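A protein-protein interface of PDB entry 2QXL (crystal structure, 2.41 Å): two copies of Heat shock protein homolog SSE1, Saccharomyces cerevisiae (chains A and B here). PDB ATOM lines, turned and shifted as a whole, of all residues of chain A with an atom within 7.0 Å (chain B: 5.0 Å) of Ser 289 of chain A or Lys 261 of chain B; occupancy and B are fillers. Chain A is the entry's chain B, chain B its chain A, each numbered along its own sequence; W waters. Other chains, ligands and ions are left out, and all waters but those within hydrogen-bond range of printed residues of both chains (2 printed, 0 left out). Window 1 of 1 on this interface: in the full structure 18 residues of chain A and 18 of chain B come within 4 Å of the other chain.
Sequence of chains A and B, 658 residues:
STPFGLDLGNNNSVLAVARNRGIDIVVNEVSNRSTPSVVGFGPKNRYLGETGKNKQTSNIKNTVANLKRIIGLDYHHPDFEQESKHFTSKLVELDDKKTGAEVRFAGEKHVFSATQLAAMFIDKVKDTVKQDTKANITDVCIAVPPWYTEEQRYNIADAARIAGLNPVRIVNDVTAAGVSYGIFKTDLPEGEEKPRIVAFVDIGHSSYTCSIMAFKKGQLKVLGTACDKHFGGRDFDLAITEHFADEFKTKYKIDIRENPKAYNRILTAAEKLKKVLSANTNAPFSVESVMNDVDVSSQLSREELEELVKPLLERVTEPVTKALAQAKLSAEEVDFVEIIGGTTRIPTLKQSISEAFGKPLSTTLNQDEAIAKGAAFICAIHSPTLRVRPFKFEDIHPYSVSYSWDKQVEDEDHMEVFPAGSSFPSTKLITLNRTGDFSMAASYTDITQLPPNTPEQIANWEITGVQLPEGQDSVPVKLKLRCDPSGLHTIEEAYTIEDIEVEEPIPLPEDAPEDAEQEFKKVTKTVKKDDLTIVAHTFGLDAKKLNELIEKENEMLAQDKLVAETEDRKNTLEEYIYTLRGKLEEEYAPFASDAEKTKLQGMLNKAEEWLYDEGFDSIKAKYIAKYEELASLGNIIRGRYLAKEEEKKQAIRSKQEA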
ATOM      1  N   ALA A 262     -33.971   0.133  18.993  1.00  0.00           N
ATOM      2  CA  ALA A 262     -32.510   0.189  19.015  1.00  0.00           C
ATOM      3  C   ALA A 262     -31.955  -0.919  19.896  1.00  0.00           C
ATOM      4  O   ALA A 262     -30.995  -1.590  19.518  1.00  0.00           O
ATOM      5  CB  ALA A 262     -32.038   1.535  19.506  1.00  0.00           C
ATOM      6  N   ARG A 265     -32.339  -4.346  18.221  1.00  0.00           N
ATOM      7  CA  ARG A 265     -31.376  -4.469  17.135  1.00  0.00           C
ATOM      8  C   ARG A 265     -30.028  -4.994  17.645  1.00  0.00           C
ATOM      9  O   ARG A 265     -29.381  -5.806  16.985  1.00  0.00           O
ATOM     10  CB  ARG A 265     -31.200  -3.120  16.414  1.00  0.00           C
ATOM     11  CG  ARG A 265     -32.357  -2.763  15.500  1.00  0.00           C
ATOM     12  CD  ARG A 265     -32.216  -1.357  14.926  1.00  0.00           C
ATOM     13  NE  ARG A 265     -33.496  -0.909  14.374  1.00  0.00           N
ATOM     14  CZ  ARG A 265     -34.126   0.228  14.671  1.00  0.00           C
ATOM     15  NH1 ARG A 265     -33.604   1.124  15.509  1.00  0.00           N
ATOM     16  NH2 ARG A 265     -35.290   0.475  14.097  1.00  0.00           N
ATOM     17  N   VAL A 287     -23.305  -3.218  13.666  1.00  0.00           N
ATOM     18  CA  VAL A 287     -24.736  -3.057  13.370  1.00  0.00           C
ATOM     19  C   VAL A 287     -24.999  -1.709  12.702  1.00  0.00           C
ATOM     20  O   VAL A 287     -24.594  -0.654  13.200  1.00  0.00           O
ATOM     21  CB  VAL A 287     -25.657  -3.207  14.627  1.00  0.00           C
ATOM     22  CG1 VAL A 287     -27.107  -3.439  14.204  1.00  0.00           C
ATOM     23  CG2 VAL A 287     -25.216  -4.343  15.504  1.00  0.00           C
ATOM     24  N   GLU A 288     -25.673  -1.757  11.560  1.00  0.00           N
ATOM     25  CA  GLU A 288     -26.031  -0.564  10.819  1.00  0.00           C
ATOM     26  C   GLU A 288     -27.308   0.071  11.377  1.00  0.00           C
ATOM     27  O   GLU A 288     -28.176  -0.642  11.866  1.00  0.00           O
ATOM     28  CB  GLU A 288     -26.180  -0.897   9.329  1.00  0.00           C
ATOM     29  CG  GLU A 288     -24.914  -1.508   8.694  1.00  0.00           C
ATOM     30  CD  GLU A 288     -24.655  -1.029   7.248  1.00  0.00           C
ATOM     31  OE1 GLU A 288     -25.637  -0.791   6.488  1.00  0.00           O
ATOM     32  OE2 GLU A 288     -23.457  -0.893   6.878  1.00  0.00           O
ATOM     33  N   SER A 289     -27.404   1.406  11.311  1.00  0.00           N
ATOM     34  CA  SER A 289     -28.593   2.180  11.741  1.00  0.00           C
ATOM     35  C   SER A 289     -29.257   1.696  13.049  1.00  0.00           C
ATOM     36  O   SER A 289     -30.464   1.441  13.081  1.00  0.00           O
ATOM     37  CB  SER A 289     -29.657   2.242  10.627  1.00  0.00           C
ATOM     38  OG  SER A 289     -29.255   3.046   9.536  1.00  0.00           O
ATOM     39  N   VAL A 290     -28.469   1.579  14.113  1.00  0.00           N
ATOM     40  CA  VAL A 290     -28.970   1.160  15.420  1.00  0.00           C
ATOM     41  C   VAL A 290     -29.984   2.161  15.951  1.00  0.00           C
ATOM     42  O   VAL A 290     -31.073   1.783  16.367  1.00  0.00           O
ATOM     43  CB  VAL A 290     -27.827   1.055  16.449  1.00  0.00           C
ATOM     44  CG1 VAL A 290     -28.348   0.540  17.787  1.00  0.00           C
ATOM     45  CG2 VAL A 290     -26.728   0.155  15.922  1.00  0.00           C
ATOM     46  N   MET A 291     -29.608   3.436  15.928  1.00  0.00           N
ATOM     47  CA  MET A 291     -30.383   4.499  16.523  1.00  0.00           C
ATOM     48  C   MET A 291     -29.980   5.785  15.843  1.00  0.00           C
ATOM     49  O   MET A 291     -28.776   6.053  15.675  1.00  0.00           O
ATOM     50  CB  MET A 291     -30.082   4.608  18.018  1.00  0.00           C
ATOM     51  CG  MET A 291     -31.192   5.254  18.838  1.00  0.00           C
ATOM     52  SD  MET A 291     -30.814   5.295  20.593  1.00  0.00           S
ATOM     53  CE  MET A 291     -29.629   4.009  20.659  1.00  0.00           C
ATOM     54  N   ASN A 292     -30.989   6.569  15.448  1.00  0.00           N
ATOM     55  CA  ASN A 292     -30.784   7.843  14.760  1.00  0.00           C
ATOM     56  C   ASN A 292     -29.879   7.696  13.533  1.00  0.00           C
ATOM     57  O   ASN A 292     -29.154   8.627  13.177  1.00  0.00           O
ATOM     58  CB  ASN A 292     -30.258   8.937  15.722  1.00  0.00           C
ATOM     59  CG  ASN A 292     -31.069   9.034  17.026  1.00  0.00           C
ATOM     60  OD1 ASN A 292     -32.250   8.679  17.085  1.00  0.00           O
ATOM     61  ND2 ASN A 292     -30.425   9.507  18.072  1.00  0.00           N
ATOM     62  N   ASP A 293     -29.936   6.521  12.899  1.00  0.00           N
ATOM     63  CA  ASP A 293     -29.136   6.198  11.703  1.00  0.00           C
ATOM     64  C   ASP A 293     -27.611   6.205  11.954  1.00  0.00           C
ATOM     65  O   ASP A 293     -26.817   6.415  11.035  1.00  0.00           O
ATOM     66  CB  ASP A 293     -29.524   7.095  10.510  1.00  0.00           C
ATOM     67  CG  ASP A 293     -30.753   6.578   9.757  1.00  0.00           C
ATOM     68  OD1 ASP A 293     -30.783   5.371   9.426  1.00  0.00           O
ATOM     69  OD2 ASP A 293     -31.684   7.374   9.479  1.00  0.00           O
ATOM     70  N   VAL A 294     -27.226   5.981  13.205  1.00  0.00           N
ATOM     71  CA  VAL A 294     -25.824   5.839  13.599  1.00  0.00           C
ATOM     72  C   VAL A 294     -25.458   4.358  13.504  1.00  0.00           C
ATOM     73  O   VAL A 294     -26.106   3.511  14.123  1.00  0.00           O
ATOM     74  CB  VAL A 294     -25.586   6.377  15.053  1.00  0.00           C
ATOM     75  CG1 VAL A 294     -24.160   6.081  15.563  1.00  0.00           C
ATOM     76  CG2 VAL A 294     -25.881   7.877  15.130  1.00  0.00           C
ATOM     77  N   ASP A 295     -24.455   4.050  12.685  1.00  0.00           N
ATOM     78  CA  ASP A 295     -23.875   2.707  12.630  1.00  0.00           C
ATOM     79  C   ASP A 295     -22.889   2.552  13.777  1.00  0.00           C
ATOM     80  O   ASP A 295     -22.119   3.467  14.075  1.00  0.00           O
ATOM     81  CB  ASP A 295     -23.117   2.468  11.314  1.00  0.00           C
ATOM     82  CG  ASP A 295     -23.984   2.639  10.081  1.00  0.00           C
ATOM     83  OD1 ASP A 295     -25.199   2.374  10.152  1.00  0.00           O
ATOM     84  OD2 ASP A 295     -23.439   3.042   9.029  1.00  0.00           O
ATOM     85  N   VAL A 296     -22.903   1.384  14.405  1.00  0.00           N
ATOM     86  CA  VAL A 296     -21.962   1.075  15.483  1.00  0.00           C
ATOM     87  C   VAL A 296     -20.982  -0.020  15.055  1.00  0.00           C
ATOM     88  O   VAL A 296     -21.309  -0.882  14.235  1.00  0.00           O
ATOM     89  CB  VAL A 296     -22.684   0.673  16.789  1.00  0.00           C
ATOM     90  CG1 VAL A 296     -23.578   1.803  17.271  1.00  0.00           C
ATOM     91  CG2 VAL A 296     -23.495  -0.585  16.581  1.00  0.00           C
ATOM     92  N   THR B  57     -30.710   3.134   0.016  1.00  0.00           N
ATOM     93  CA  THR B  57     -30.867   3.903   1.248  1.00  0.00           C
ATOM     94  C   THR B  57     -29.731   3.564   2.198  1.00  0.00           C
ATOM     95  O   THR B  57     -29.079   4.464   2.726  1.00  0.00           O
ATOM     96  CB  THR B  57     -32.269   3.726   1.892  1.00  0.00           C
ATOM     97  OG1 THR B  57     -33.264   4.226   0.986  1.00  0.00           O
ATOM     98  CG2 THR B  57     -32.379   4.495   3.194  1.00  0.00           C
ATOM     99  N   SER B  58     -29.468   2.274   2.378  1.00  0.00           N
ATOM    100  CA  SER B  58     -28.409   1.837   3.274  1.00  0.00           C
ATOM    101  C   SER B  58     -27.007   2.230   2.790  1.00  0.00           C
ATOM    102  O   SER B  58     -26.149   2.526   3.608  1.00  0.00           O
ATOM    103  CB  SER B  58     -28.510   0.332   3.564  1.00  0.00           C
ATOM    104  OG  SER B  58     -28.248  -0.426   2.411  1.00  0.00           O
ATOM    105  N   ILE B  60     -26.442   4.925   0.735  1.00  0.00           N
ATOM    106  CA  ILE B  60     -26.844   6.208   0.117  1.00  0.00           C
ATOM    107  C   ILE B  60     -25.709   7.018  -0.547  1.00  0.00           C
ATOM    108  O   ILE B  60     -25.858   7.475  -1.677  1.00  0.00           O
ATOM    109  CB  ILE B  60     -27.736   7.081   1.109  1.00  0.00           C
ATOM    110  CG1 ILE B  60     -28.326   8.313   0.439  1.00  0.00           C
ATOM    111  CG2 ILE B  60     -26.986   7.509   2.368  1.00  0.00           C
ATOM    112  CD1 ILE B  60     -29.755   8.184   0.063  1.00  0.00           C
ATOM    113  N   ASN B 259     -31.073  14.480   7.190  1.00  0.00           N
ATOM    114  CA  ASN B 259     -30.731  13.057   7.242  1.00  0.00           C
ATOM    115  C   ASN B 259     -31.033  12.464   5.881  1.00  0.00           C
ATOM    116  O   ASN B 259     -32.195  12.195   5.569  1.00  0.00           O
ATOM    117  CB  ASN B 259     -31.514  12.347   8.359  1.00  0.00           C
ATOM    118  CG  ASN B 259     -31.209  10.839   8.462  1.00  0.00           C
ATOM    119  OD1 ASN B 259     -30.734  10.196   7.519  1.00  0.00           O
ATOM    120  ND2 ASN B 259     -31.507  10.275   9.615  1.00  0.00           N
ATOM    121  N   PRO B 260     -29.986  12.275   5.057  1.00  0.00           N
ATOM    122  CA  PRO B 260     -30.149  11.800   3.677  1.00  0.00           C
ATOM    123  C   PRO B 260     -30.915  10.486   3.576  1.00  0.00           C
ATOM    124  O   PRO B 260     -31.639  10.288   2.606  1.00  0.00           O
ATOM    125  CB  PRO B 260     -28.704  11.628   3.187  1.00  0.00           C
ATOM    126  CG  PRO B 260     -27.896  12.555   4.065  1.00  0.00           C
ATOM    127  CD  PRO B 260     -28.566  12.508   5.402  1.00  0.00           C
ATOM    128  N   LYS B 261     -30.763   9.598   4.561  1.00  0.00           N
ATOM    129  CA  LYS B 261     -31.501   8.324   4.564  1.00  0.00           C
ATOM    130  C   LYS B 261     -33.009   8.505   4.803  1.00  0.00           C
ATOM    131  O   LYS B 261     -33.824   7.902   4.101  1.00  0.00           O
ATOM    132  CB  LYS B 261     -30.901   7.336   5.563  1.00  0.00           C
ATOM    133  CG  LYS B 261     -29.567   6.778   5.114  1.00  0.00           C
ATOM    134  CD  LYS B 261     -29.121   5.589   5.975  1.00  0.00           C
ATOM    135  CE  LYS B 261     -27.646   5.304   5.742  1.00  0.00           C
ATOM    136  NZ  LYS B 261     -27.215   3.972   6.253  1.00  0.00           N
ATOM    137  N   ALA B 262     -33.359   9.335   5.788  1.00  0.00           N
ATOM    138  CA  ALA B 262     -34.748   9.723   6.047  1.00  0.00           C
ATOM    139  C   ALA B 262     -35.393  10.316   4.799  1.00  0.00           C
ATOM    140  O   ALA B 262     -36.515   9.958   4.444  1.00  0.00           O
ATOM    141  CB  ALA B 262     -34.825  10.700   7.197  1.00  0.00           C
ATOM    142  N   TYR B 263     -34.664  11.202   4.127  1.00  0.00           N
ATOM    143  CA  TYR B 263     -35.165  11.901   2.953  1.00  0.00           C
ATOM    144  C   TYR B 263     -35.480  10.909   1.838  1.00  0.00           C
ATOM    145  O   TYR B 263     -36.546  10.967   1.223  1.00  0.00           O
ATOM    146  CB  TYR B 263     -34.157  12.970   2.493  1.00  0.00           C
ATOM    147  CG  TYR B 263     -34.744  13.963   1.508  1.00  0.00           C
ATOM    148  CD1 TYR B 263     -35.423  15.091   1.952  1.00  0.00           C
ATOM    149  CD2 TYR B 263     -34.644  13.752   0.125  1.00  0.00           C
ATOM    150  CE1 TYR B 263     -35.978  16.005   1.053  1.00  0.00           C
ATOM    151  CE2 TYR B 263     -35.195  14.666  -0.785  1.00  0.00           C
ATOM    152  CZ  TYR B 263     -35.861  15.782  -0.306  1.00  0.00           C
ATOM    153  OH  TYR B 263     -36.417  16.682  -1.194  1.00  0.00           O
ATOM    154  N   ASN B 264     -34.557   9.975   1.622  1.00  0.00           N
ATOM    155  CA  ASN B 264     -34.700   8.942   0.611  1.00  0.00           C
ATOM    156  C   ASN B 264     -35.815   7.921   0.897  1.00  0.00           C
ATOM    157  O   ASN B 264     -36.389   7.346  -0.033  1.00  0.00           O
ATOM    158  CB  ASN B 264     -33.371   8.216   0.425  1.00  0.00           C
ATOM    159  CG  ASN B 264     -33.263   7.559  -0.932  1.00  0.00           C
ATOM    160  OD1 ASN B 264     -33.197   8.241  -1.954  1.00  0.00           O
ATOM    161  ND2 ASN B 264     -33.266   6.239  -0.955  1.00  0.00           N
ATOM    162  N   ARG B 265     -36.096   7.690   2.175  1.00  0.00           N
ATOM    163  CA  ARG B 265     -37.233   6.876   2.595  1.00  0.00           C
ATOM    164  C   ARG B 265     -38.555   7.558   2.233  1.00  0.00           C
ATOM    165  O   ARG B 265     -39.504   6.903   1.836  1.00  0.00           O
ATOM    166  CB  ARG B 265     -37.183   6.602   4.110  1.00  0.00           C
ATOM    167  CG  ARG B 265     -36.051   5.688   4.540  1.00  0.00           C
ATOM    168  CD  ARG B 265     -35.949   5.620   6.071  1.00  0.00           C
ATOM    169  NE  ARG B 265     -34.767   4.881   6.504  1.00  0.00           N
ATOM    170  CZ  ARG B 265     -33.813   5.354   7.309  1.00  0.00           C
ATOM    171  NH1 ARG B 265     -33.876   6.591   7.803  1.00  0.00           N
ATOM    172  NH2 ARG B 265     -32.784   4.573   7.633  1.00  0.00           N
HETATM  173  O   HOH W   1     -32.505   8.480  11.902  1.00  0.00           O
HETATM  174  O   HOH W   2     -31.498  11.103  12.476  1.00  0.00           O
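The side-chain carboxylate (OD1) of Asp 293 of chain A is in salt-bridge range of the guanidinium group (NH2) of Arg 265 of chain B, at 2.8 Å.
The side-chain amide nitrogen of Asn 259 of chain B lies within hydrogen-bond range of the side-chain carboxylate of Asp 293 of chain A (2.9 Å).
The side-chain amide oxygen (OD1) of Asn 259 of chain B sits at hydrogen-bond distance from the backbone NH (N) of Ala 262 of chain B (3.3 Å).
The backbone carbonyl oxygen of Ser 58 of chain B lies within hydrogen-bond range of the side-chain amino group of Lys 261 of chain B.
OD1 of Asp 293 of chain A lies within hydrogen-bond range of OG of Ser 289 of chain A.
The side-chain amide oxygen (OD1) of Asn 259 of chain B sits at hydrogen-bond distance from the backbone NH (N) of Lys 261 of chain B (3.0 Å).
The side-chain carboxylate (OD1) of Asp 295 of chain A lies within hydrogen-bond range of the backbone NH (N) of Ser 289 of chain A, 2.7 Å away.
Ser 289 of chain A touches Lys 261 of chain B (OG to NZ, 3.97 Å).
Asp 293 of chain A touches Lys 261 of chain B.
Of chain B, only Lys 261 comes within 4 Å of Ser 289 of chain A.
Of the printed residues of chain A, Lys 261 of chain B touches Ser 289 and Asp 293.
Printed residues of chain A within 4 Å of Arg 265 of chain B: Asp 293 (2.8 Å).
Printed residues of chain A within 4 Å of Asn 259 of chain B: Asp 293 (2.9 Å).
Of the printed residues of chain B, Asp 293 of chain A touches Asn 259 (2.9 Å), Lys 261 (3.8 Å) and Arg 265 (2.8 Å).
Val 296 of chain A touches none of the printed residues of chain B.
Of the 12 printed residues of chain A, 2 touch a printed residue of chain B.
Printed residues of chain B that touch a printed residue of chain A: Asn 259, Lys 261 and Arg 265.
Among the printed residues, 4 pairs touch across the chains.
Positions printed for both chains: 262 and 265.
Of the 4 pairs that touch across the chains among the printed residues, none has its exchanged pair printed and touching as well.
Water W1 bridges OD2 of Asp 293 of chain A (2.8 Å) and ND2 of Asn 259 of chain B (3.1 Å).
Water W2 lies within hydrogen-bond range of the side-chain amide nitrogen (ND2) of Asn 259 of chain B and the backbone carbonyl oxygen (O) of Asn 292 of chain A.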
